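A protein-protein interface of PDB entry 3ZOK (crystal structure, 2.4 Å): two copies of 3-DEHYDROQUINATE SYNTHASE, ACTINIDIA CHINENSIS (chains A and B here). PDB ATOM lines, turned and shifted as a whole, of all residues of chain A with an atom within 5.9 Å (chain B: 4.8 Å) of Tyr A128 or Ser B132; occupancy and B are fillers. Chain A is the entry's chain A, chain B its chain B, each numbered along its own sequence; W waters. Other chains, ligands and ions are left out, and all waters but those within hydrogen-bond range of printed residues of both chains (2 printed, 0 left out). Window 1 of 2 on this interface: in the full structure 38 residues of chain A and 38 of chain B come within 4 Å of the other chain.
The backbone carbonyl oxygen (O) of Leu A168 is in hydrogen-bond range of the backbone NH (N) of Leu B134 (2.8 Å). OH of Tyr B128 sits at hydrogen-bond distance from OG of Ser A132 (2.8 Å). The side-chain hydroxyl of Tyr B128 lies within hydrogen-bond range of the side-chain hydroxyl of Tyr A128 (2.9 Å). The guanidinium group (NE) of Arg B135 lies within hydrogen-bond range of the backbone carbonyl oxygen (O) of Thr A158, at 3.0 Å. The backbone carbonyl oxygen (O) of Ser B132 lies within hydrogen-bond range of the backbone NH (N) of Gly A170 (3.0 Å). The side-chain hydroxyl (OG) of Ser B132 sits at hydrogen-bond distance from the side-chain hydroxyl (OH) of Tyr A128.
N of Ile A160 is in hydrogen-bond range of O of Ile A169 (2.7 Å). The side-chain hydroxyl of Thr A158 lies within hydrogen-bond range of the backbone carbonyl oxygen of Ala A171 (2.7 Å). The backbone carbonyl oxygen of Ile A160 lies within hydrogen-bond range of the backbone NH of Leu A168 (3.1 Å). O of Tyr B128 lies within hydrogen-bond range of OG of Ser B132 (3.2 Å). O of Tyr A128 lies close to OG of Ser A132, at 3.4 Å. N of Gly B136 sits at hydrogen-bond distance from O of Ala B131.
Among the printed residues, pairs that only touch across the chains: Ile A169 with Ser B132, Ile A169 with Phe B100, Gly A170 with Arg B135, Leu A168 with Ser B132, Leu A168 with Phe B133, Ala A171 with Arg B135 and Gly A170 with Ala B131.
Asp A124 touches none of the printed residues of chain B. Of the printed residues of chain B, Thr A158 touches Arg B135. Of the printed residues of chain B, Gly A170 touches Ala B131 (3.9 Å), Ser B132 (3.0 Å) and Arg B135 (3.6 Å). Printed residues of chain B within 4 Å of Ala A171: Arg B135 (3.8 Å). Printed residues of chain A within 4 Å of Ser B132: Tyr A128 (3.0 Å), Leu A168 (3.8 Å), Ile A169 (3.4 Å) and Gly A170 (3.0 Å). Of the printed residues of chain A, Phe B133 touches Leu A168. Of the printed residues of chain A, Leu B134 touches Leu A168 (2.8 Å).
Of the 21 printed residues of chain A, 7 touch a printed residue of chain B. Hydrophobic or aromatic side chains of chain A within 4 Å of the printed part of chain B: Tyr A128, Leu A168 and Ile A169. Hydrophobic or aromatic side chains of chain B within 4 Å of the printed part of chain A: Phe B100, Tyr B128, Phe B133 and Leu B134. Among the printed residues, no Asp or Glu carboxylate lies within 4 Å of a Lys or Arg side-chain nitrogen of the other chain.
Tyr A128 touches its own counterpart, Tyr B128. Tyr A128 touches Ser B132, and with the chains exchanged Ser A132 touches Tyr B128. 7 positions are printed for both chains. Of the 13 pairs that touch across the chains among the printed residues, 3 have their exchanged pair printed and touching as well.
Water W1 lies within hydrogen-bond range of NH2 of Arg B135, OD2 of Asp A124, N of Gly A159 and O of Thr A158. Water W2 lies within hydrogen-bond range of the side-chain hydroxyl (OG) of Ser B132 (2.7 Å), the backbone carbonyl oxygen (O) of Gly A170 (2.9 Å) and the backbone carbonyl oxygen (O) of Ala B131 (3.3 Å).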
ATOM      1  N   MET A  93      12.690  30.127   3.666  1.00  0.00           N
ATOM      2  CA  MET A  93      11.985  31.010   2.786  1.00  0.00           C
ATOM      3  C   MET A  93      12.665  31.140   1.404  1.00  0.00           C
ATOM      4  O   MET A  93      11.991  31.281   0.383  1.00  0.00           O
ATOM      5  CB  MET A  93      11.835  32.373   3.444  1.00  0.00           C
ATOM      6  CG  MET A  93      10.927  33.324   2.694  1.00  0.00           C
ATOM      7  SD  MET A  93       9.229  32.750   2.781  1.00  0.00           S
ATOM      8  CE  MET A  93       9.160  32.066   1.160  1.00  0.00           C
ATOM      9  N   LEU A  96      11.900  28.075  -0.668  1.00  0.00           N
ATOM     10  CA  LEU A  96      10.493  28.147  -1.039  1.00  0.00           C
ATOM     11  C   LEU A  96      10.249  29.133  -2.180  1.00  0.00           C
ATOM     12  O   LEU A  96       9.386  28.916  -3.035  1.00  0.00           O
ATOM     13  CB  LEU A  96       9.623  28.541   0.158  1.00  0.00           C
ATOM     14  CG  LEU A  96       8.102  28.432  -0.076  1.00  0.00           C
ATOM     15  CD1 LEU A  96       7.500  27.138   0.401  1.00  0.00           C
ATOM     16  CD2 LEU A  96       7.366  29.572   0.589  1.00  0.00           C
ATOM     17  N   PHE A 100       7.780  29.451  -6.045  1.00  0.00           N
ATOM     18  CA  PHE A 100       6.985  30.557  -6.590  1.00  0.00           C
ATOM     19  C   PHE A 100       7.583  31.104  -7.882  1.00  0.00           C
ATOM     20  O   PHE A 100       6.848  31.436  -8.791  1.00  0.00           O
ATOM     21  CB  PHE A 100       6.895  31.711  -5.609  1.00  0.00           C
ATOM     22  CG  PHE A 100       6.206  31.379  -4.328  1.00  0.00           C
ATOM     23  CD1 PHE A 100       4.948  30.765  -4.323  1.00  0.00           C
ATOM     24  CD2 PHE A 100       6.786  31.748  -3.116  1.00  0.00           C
ATOM     25  CE1 PHE A 100       4.305  30.490  -3.113  1.00  0.00           C
ATOM     26  CE2 PHE A 100       6.159  31.476  -1.931  1.00  0.00           C
ATOM     27  CZ  PHE A 100       4.914  30.850  -1.924  1.00  0.00           C
ATOM     28  N   GLY A 123       7.062  17.898   1.418  1.00  0.00           N
ATOM     29  CA  GLY A 123       5.652  18.017   1.655  1.00  0.00           C
ATOM     30  C   GLY A 123       5.326  19.343   2.285  1.00  0.00           C
ATOM     31  O   GLY A 123       4.367  20.045   1.874  1.00  0.00           O
ATOM     32  N   ASP A 124       6.116  19.684   3.305  1.00  0.00           N
ATOM     33  CA  ASP A 124       5.840  20.891   4.069  1.00  0.00           C
ATOM     34  C   ASP A 124       6.069  22.121   3.175  1.00  0.00           C
ATOM     35  O   ASP A 124       5.244  23.038   3.140  1.00  0.00           O
ATOM     36  CB  ASP A 124       6.692  20.950   5.338  1.00  0.00           C
ATOM     37  CG  ASP A 124       6.138  20.105   6.465  1.00  0.00           C
ATOM     38  OD1 ASP A 124       5.167  19.335   6.258  1.00  0.00           O
ATOM     39  OD2 ASP A 124       6.675  20.219   7.587  1.00  0.00           O
ATOM     40  N   MET A 125       7.174  22.118   2.430  1.00  0.00           N
ATOM     41  CA  MET A 125       7.499  23.261   1.603  1.00  0.00           C
ATOM     42  C   MET A 125       6.466  23.418   0.489  1.00  0.00           C
ATOM     43  O   MET A 125       6.025  24.528   0.165  1.00  0.00           O
ATOM     44  CB  MET A 125       8.907  23.106   1.033  1.00  0.00           C
ATOM     45  CG  MET A 125      10.011  23.179   2.078  1.00  0.00           C
ATOM     46  SD  MET A 125      11.568  23.897   1.500  1.00  0.00           S
ATOM     47  CE  MET A 125      10.933  25.421   0.854  1.00  0.00           C
ATOM     48  N   CYS A 126       6.061  22.280  -0.069  1.00  0.00           N
ATOM     49  CA  CYS A 126       5.195  22.265  -1.216  1.00  0.00           C
ATOM     50  C   CYS A 126       3.816  22.682  -0.843  1.00  0.00           C
ATOM     51  O   CYS A 126       3.140  23.397  -1.583  1.00  0.00           O
ATOM     52  CB  CYS A 126       5.155  20.873  -1.810  1.00  0.00           C
ATOM     53  SG  CYS A 126       4.229  20.835  -3.346  1.00  0.00           S
ATOM     54  N   GLY A 127       3.381  22.205   0.308  1.00  0.00           N
ATOM     55  CA  GLY A 127       2.054  22.493   0.808  1.00  0.00           C
ATOM     56  C   GLY A 127       1.903  23.979   1.071  1.00  0.00           C
ATOM     57  O   GLY A 127       0.822  24.542   0.814  1.00  0.00           O
ATOM     58  N   TYR A 128       2.957  24.606   1.623  1.00  0.00           N
ATOM     59  CA  TYR A 128       2.875  26.023   1.980  1.00  0.00           C
ATOM     60  C   TYR A 128       2.892  26.918   0.722  1.00  0.00           C
ATOM     61  O   TYR A 128       2.124  27.883   0.610  1.00  0.00           O
ATOM     62  CB  TYR A 128       3.981  26.414   2.988  1.00  0.00           C
ATOM     63  CG  TYR A 128       4.043  27.894   3.333  1.00  0.00           C
ATOM     64  CD1 TYR A 128       2.883  28.676   3.461  1.00  0.00           C
ATOM     65  CD2 TYR A 128       5.259  28.507   3.573  1.00  0.00           C
ATOM     66  CE1 TYR A 128       2.956  30.028   3.781  1.00  0.00           C
ATOM     67  CE2 TYR A 128       5.339  29.853   3.910  1.00  0.00           C
ATOM     68  CZ  TYR A 128       4.195  30.611   3.999  1.00  0.00           C
ATOM     69  OH  TYR A 128       4.319  31.945   4.301  1.00  0.00           O
ATOM     70  N   ALA A 129       3.757  26.552  -0.223  1.00  0.00           N
ATOM     71  CA  ALA A 129       3.824  27.187  -1.517  1.00  0.00           C
ATOM     72  C   ALA A 129       2.465  27.156  -2.192  1.00  0.00           C
ATOM     73  O   ALA A 129       1.986  28.195  -2.690  1.00  0.00           O
ATOM     74  CB  ALA A 129       4.849  26.482  -2.385  1.00  0.00           C
ATOM     75  N   ALA A 130       1.858  25.969  -2.202  1.00  0.00           N
ATOM     76  CA  ALA A 130       0.538  25.765  -2.753  1.00  0.00           C
ATOM     77  C   ALA A 130      -0.496  26.618  -2.049  1.00  0.00           C
ATOM     78  O   ALA A 130      -1.363  27.213  -2.689  1.00  0.00           O
ATOM     79  CB  ALA A 130       0.153  24.302  -2.640  1.00  0.00           C
ATOM     80  N   ALA A 131      -0.426  26.676  -0.722  1.00  0.00           N
ATOM     81  CA  ALA A 131      -1.360  27.512   0.032  1.00  0.00           C
ATOM     82  C   ALA A 131      -1.280  28.968  -0.437  1.00  0.00           C
ATOM     83  O   ALA A 131      -2.300  29.661  -0.492  1.00  0.00           O
ATOM     84  CB  ALA A 131      -1.084  27.449   1.527  1.00  0.00           C
ATOM     85  N   SER A 132      -0.055  29.409  -0.729  1.00  0.00           N
ATOM     86  CA  SER A 132       0.231  30.807  -0.868  1.00  0.00           C
ATOM     87  C   SER A 132       0.224  31.248  -2.318  1.00  0.00           C
ATOM     88  O   SER A 132      -0.126  32.376  -2.595  1.00  0.00           O
ATOM     89  CB  SER A 132       1.566  31.137  -0.210  1.00  0.00           C
ATOM     90  OG  SER A 132       1.469  31.153   1.211  1.00  0.00           O
ATOM     91  N   PHE A 133       0.585  30.370  -3.243  1.00  0.00           N
ATOM     92  CA  PHE A 133       0.682  30.756  -4.628  1.00  0.00           C
ATOM     93  C   PHE A 133      -0.702  31.135  -5.141  1.00  0.00           C
ATOM     94  O   PHE A 133      -1.641  30.325  -5.086  1.00  0.00           O
ATOM     95  CB  PHE A 133       1.286  29.640  -5.468  1.00  0.00           C
ATOM     96  CG  PHE A 133       1.378  29.965  -6.941  1.00  0.00           C
ATOM     97  CD1 PHE A 133       2.005  31.123  -7.368  1.00  0.00           C
ATOM     98  CD2 PHE A 133       0.868  29.087  -7.900  1.00  0.00           C
ATOM     99  CE1 PHE A 133       2.079  31.430  -8.698  1.00  0.00           C
ATOM    100  CE2 PHE A 133       0.966  29.380  -9.253  1.00  0.00           C
ATOM    101  CZ  PHE A 133       1.569  30.566  -9.649  1.00  0.00           C
ATOM    102  N   THR A 158       1.602  22.776   6.972  1.00  0.00           N
ATOM    103  CA  THR A 158       2.687  23.081   6.059  1.00  0.00           C
ATOM    104  C   THR A 158       3.530  24.261   6.569  1.00  0.00           C
ATOM    105  O   THR A 158       3.108  25.041   7.461  1.00  0.00           O
ATOM    106  CB  THR A 158       2.124  23.511   4.707  1.00  0.00           C
ATOM    107  OG1 THR A 158       1.564  24.826   4.842  1.00  0.00           O
ATOM    108  CG2 THR A 158       1.048  22.512   4.219  1.00  0.00           C
ATOM    109  N   GLY A 159       4.720  24.396   6.001  1.00  0.00           N
ATOM    110  CA  GLY A 159       5.531  25.564   6.260  1.00  0.00           C
ATOM    111  C   GLY A 159       7.027  25.332   6.280  1.00  0.00           C
ATOM    112  O   GLY A 159       7.536  24.273   5.853  1.00  0.00           O
ATOM    113  N   ILE A 160       7.718  26.350   6.802  1.00  0.00           N
ATOM    114  CA  ILE A 160       9.154  26.402   6.838  1.00  0.00           C
ATOM    115  C   ILE A 160       9.664  26.717   8.248  1.00  0.00           C
ATOM    116  O   ILE A 160       8.929  27.214   9.097  1.00  0.00           O
ATOM    117  CB  ILE A 160       9.677  27.440   5.827  1.00  0.00           C
ATOM    118  CG1 ILE A 160       8.967  28.785   5.987  1.00  0.00           C
ATOM    119  CG2 ILE A 160       9.463  26.932   4.409  1.00  0.00           C
ATOM    120  CD1 ILE A 160       9.637  29.943   5.263  1.00  0.00           C
ATOM    121  N   LEU A 168       7.883  27.928  11.975  1.00  0.00           N
ATOM    122  CA  LEU A 168       7.330  29.171  12.513  1.00  0.00           C
ATOM    123  C   LEU A 168       6.573  29.995  11.473  1.00  0.00           C
ATOM    124  O   LEU A 168       5.904  30.999  11.791  1.00  0.00           O
ATOM    125  CB  LEU A 168       8.452  29.978  13.167  1.00  0.00           C
ATOM    126  CG  LEU A 168       9.112  29.275  14.373  1.00  0.00           C
ATOM    127  CD1 LEU A 168      10.088  30.217  15.072  1.00  0.00           C
ATOM    128  CD2 LEU A 168       8.059  28.846  15.365  1.00  0.00           C
ATOM    129  N   ILE A 169       6.678  29.573  10.231  1.00  0.00           N
ATOM    130  CA  ILE A 169       6.020  30.251   9.150  1.00  0.00           C
ATOM    131  C   ILE A 169       5.400  29.185   8.274  1.00  0.00           C
ATOM    132  O   ILE A 169       6.086  28.228   7.871  1.00  0.00           O
ATOM    133  CB  ILE A 169       7.008  31.064   8.288  1.00  0.00           C
ATOM    134  CG1 ILE A 169       7.820  32.038   9.161  1.00  0.00           C
ATOM    135  CG2 ILE A 169       6.262  31.784   7.166  1.00  0.00           C
ATOM    136  CD1 ILE A 169       8.808  32.874   8.371  1.00  0.00           C
ATOM    137  N   GLY A 170       4.118  29.362   7.959  1.00  0.00           N
ATOM    138  CA  GLY A 170       3.423  28.373   7.150  1.00  0.00           C
ATOM    139  C   GLY A 170       1.929  28.555   7.045  1.00  0.00           C
ATOM    140  O   GLY A 170       1.422  29.672   7.073  1.00  0.00           O
ATOM    141  N   ALA A 171       1.217  27.448   6.876  1.00  0.00           N
ATOM    142  CA  ALA A 171      -0.213  27.527   6.641  1.00  0.00           C
ATOM    143  C   ALA A 171      -0.862  26.214   6.935  1.00  0.00           C
ATOM    144  O   ALA A 171      -0.232  25.173   6.760  1.00  0.00           O
ATOM    145  CB  ALA A 171      -0.483  27.922   5.201  1.00  0.00           C
ATOM    146  N   PHE B 100       8.245  38.794  10.535  1.00  0.00           N
ATOM    147  CA  PHE B 100       8.517  37.493  11.159  1.00  0.00           C
ATOM    148  C   PHE B 100       9.688  37.565  12.101  1.00  0.00           C
ATOM    149  O   PHE B 100       9.607  37.089  13.229  1.00  0.00           O
ATOM    150  CB  PHE B 100       8.781  36.387  10.131  1.00  0.00           C
ATOM    151  CG  PHE B 100       7.656  36.176   9.160  1.00  0.00           C
ATOM    152  CD1 PHE B 100       6.357  36.003   9.609  1.00  0.00           C
ATOM    153  CD2 PHE B 100       7.894  36.185   7.800  1.00  0.00           C
ATOM    154  CE1 PHE B 100       5.314  35.835   8.718  1.00  0.00           C
ATOM    155  CE2 PHE B 100       6.860  36.007   6.913  1.00  0.00           C
ATOM    156  CZ  PHE B 100       5.568  35.828   7.376  1.00  0.00           C
ATOM    157  N   TYR B 128      -1.002  39.089   5.448  1.00  0.00           N
ATOM    158  CA  TYR B 128      -0.346  37.873   5.010  1.00  0.00           C
ATOM    159  C   TYR B 128       0.699  37.388   6.040  1.00  0.00           C
ATOM    160  O   TYR B 128       0.910  36.189   6.209  1.00  0.00           O
ATOM    161  CB  TYR B 128       0.260  38.029   3.589  1.00  0.00           C
ATOM    162  CG  TYR B 128       0.980  36.779   3.165  1.00  0.00           C
ATOM    163  CD1 TYR B 128       0.326  35.549   3.155  1.00  0.00           C
ATOM    164  CD2 TYR B 128       2.301  36.805   2.837  1.00  0.00           C
ATOM    165  CE1 TYR B 128       0.971  34.395   2.793  1.00  0.00           C
ATOM    166  CE2 TYR B 128       2.959  35.636   2.491  1.00  0.00           C
ATOM    167  CZ  TYR B 128       2.282  34.439   2.478  1.00  0.00           C
ATOM    168  OH  TYR B 128       2.938  33.317   2.151  1.00  0.00           O
ATOM    169  N   ALA B 129       1.331  38.327   6.742  1.00  0.00           N
ATOM    170  CA  ALA B 129       2.259  37.994   7.822  1.00  0.00           C
ATOM    171  C   ALA B 129       1.500  37.303   8.938  1.00  0.00           C
ATOM    172  O   ALA B 129       1.999  36.326   9.539  1.00  0.00           O
ATOM    173  CB  ALA B 129       2.916  39.255   8.357  1.00  0.00           C
ATOM    174  N   ALA B 130       0.313  37.822   9.239  1.00  0.00           N
ATOM    175  CA  ALA B 130      -0.512  37.196  10.286  1.00  0.00           C
ATOM    176  C   ALA B 130      -0.998  35.807   9.899  1.00  0.00           C
ATOM    177  O   ALA B 130      -0.969  34.879  10.722  1.00  0.00           O
ATOM    178  CB  ALA B 130      -1.692  38.073  10.665  1.00  0.00           C
ATOM    179  N   ALA B 131      -1.426  35.672   8.646  1.00  0.00           N
ATOM    180  CA  ALA B 131      -1.898  34.388   8.120  1.00  0.00           C
ATOM    181  C   ALA B 131      -0.839  33.317   8.281  1.00  0.00           C
ATOM    182  O   ALA B 131      -1.178  32.167   8.501  1.00  0.00           O
ATOM    183  CB  ALA B 131      -2.278  34.506   6.651  1.00  0.00           C
ATOM    184  N   SER B 132       0.431  33.722   8.151  1.00  0.00           N
ATOM    185  CA  SER B 132       1.548  32.811   8.049  1.00  0.00           C
ATOM    186  C   SER B 132       2.317  32.673   9.323  1.00  0.00           C
ATOM    187  O   SER B 132       2.975  31.649   9.521  1.00  0.00           O
ATOM    188  CB  SER B 132       2.529  33.261   6.966  1.00  0.00           C
ATOM    189  OG  SER B 132       1.944  33.200   5.690  1.00  0.00           O
ATOM    190  N   PHE B 133       2.279  33.694  10.181  1.00  0.00           N
ATOM    191  CA  PHE B 133       3.041  33.603  11.405  1.00  0.00           C
ATOM    192  C   PHE B 133       2.419  32.474  12.229  1.00  0.00           C
ATOM    193  O   PHE B 133       1.226  32.515  12.560  1.00  0.00           O
ATOM    194  CB  PHE B 133       3.111  34.924  12.166  1.00  0.00           C
ATOM    195  CG  PHE B 133       3.907  34.843  13.440  1.00  0.00           C
ATOM    196  CD1 PHE B 133       5.198  34.312  13.443  1.00  0.00           C
ATOM    197  CD2 PHE B 133       3.374  35.264  14.613  1.00  0.00           C
ATOM    198  CE1 PHE B 133       5.941  34.210  14.607  1.00  0.00           C
ATOM    199  CE2 PHE B 133       4.093  35.166  15.777  1.00  0.00           C
ATOM    200  CZ  PHE B 133       5.390  34.637  15.780  1.00  0.00           C
ATOM    201  N   LEU B 134       3.246  31.441  12.472  1.00  0.00           N
ATOM    202  CA  LEU B 134       2.883  30.243  13.244  1.00  0.00           C
ATOM    203  C   LEU B 134       1.682  29.541  12.643  1.00  0.00           C
ATOM    204  O   LEU B 134       0.992  28.812  13.334  1.00  0.00           O
ATOM    205  CB  LEU B 134       2.635  30.596  14.702  1.00  0.00           C
ATOM    206  CG  LEU B 134       3.684  31.488  15.365  1.00  0.00           C
ATOM    207  CD1 LEU B 134       3.273  31.855  16.785  1.00  0.00           C
ATOM    208  CD2 LEU B 134       5.066  30.845  15.344  1.00  0.00           C
ATOM    209  N   ARG B 135       1.484  29.750  11.331  1.00  0.00           N
ATOM    210  CA  ARG B 135       0.359  29.241  10.520  1.00  0.00           C
ATOM    211  C   ARG B 135      -0.961  29.934  10.805  1.00  0.00           C
ATOM    212  O   ARG B 135      -2.039  29.406  10.457  1.00  0.00           O
ATOM    213  CB  ARG B 135       0.150  27.740  10.640  1.00  0.00           C
ATOM    214  CG  ARG B 135       1.395  26.885  10.613  1.00  0.00           C
ATOM    215  CD  ARG B 135       0.982  25.452  10.350  1.00  0.00           C
ATOM    216  NE  ARG B 135       2.122  24.574  10.203  1.00  0.00           N
ATOM    217  CZ  ARG B 135       2.697  23.887  11.186  1.00  0.00           C
ATOM    218  NH1 ARG B 135       2.254  23.956  12.434  1.00  0.00           N
ATOM    219  NH2 ARG B 135       3.732  23.116  10.899  1.00  0.00           N
ATOM    220  N   GLY B 136      -0.889  31.112  11.412  1.00  0.00           N
ATOM    221  CA  GLY B 136      -2.067  31.967  11.551  1.00  0.00           C
ATOM    222  C   GLY B 136      -2.232  32.526  12.947  1.00  0.00           C
ATOM    223  O   GLY B 136      -2.587  31.797  13.872  1.00  0.00           O
HETATM  224  O   HOH W   1       4.574  22.231   8.550  1.00  0.00           O
HETATM  225  O   HOH W   2      -0.119  31.544   5.459  1.00  0.00           O
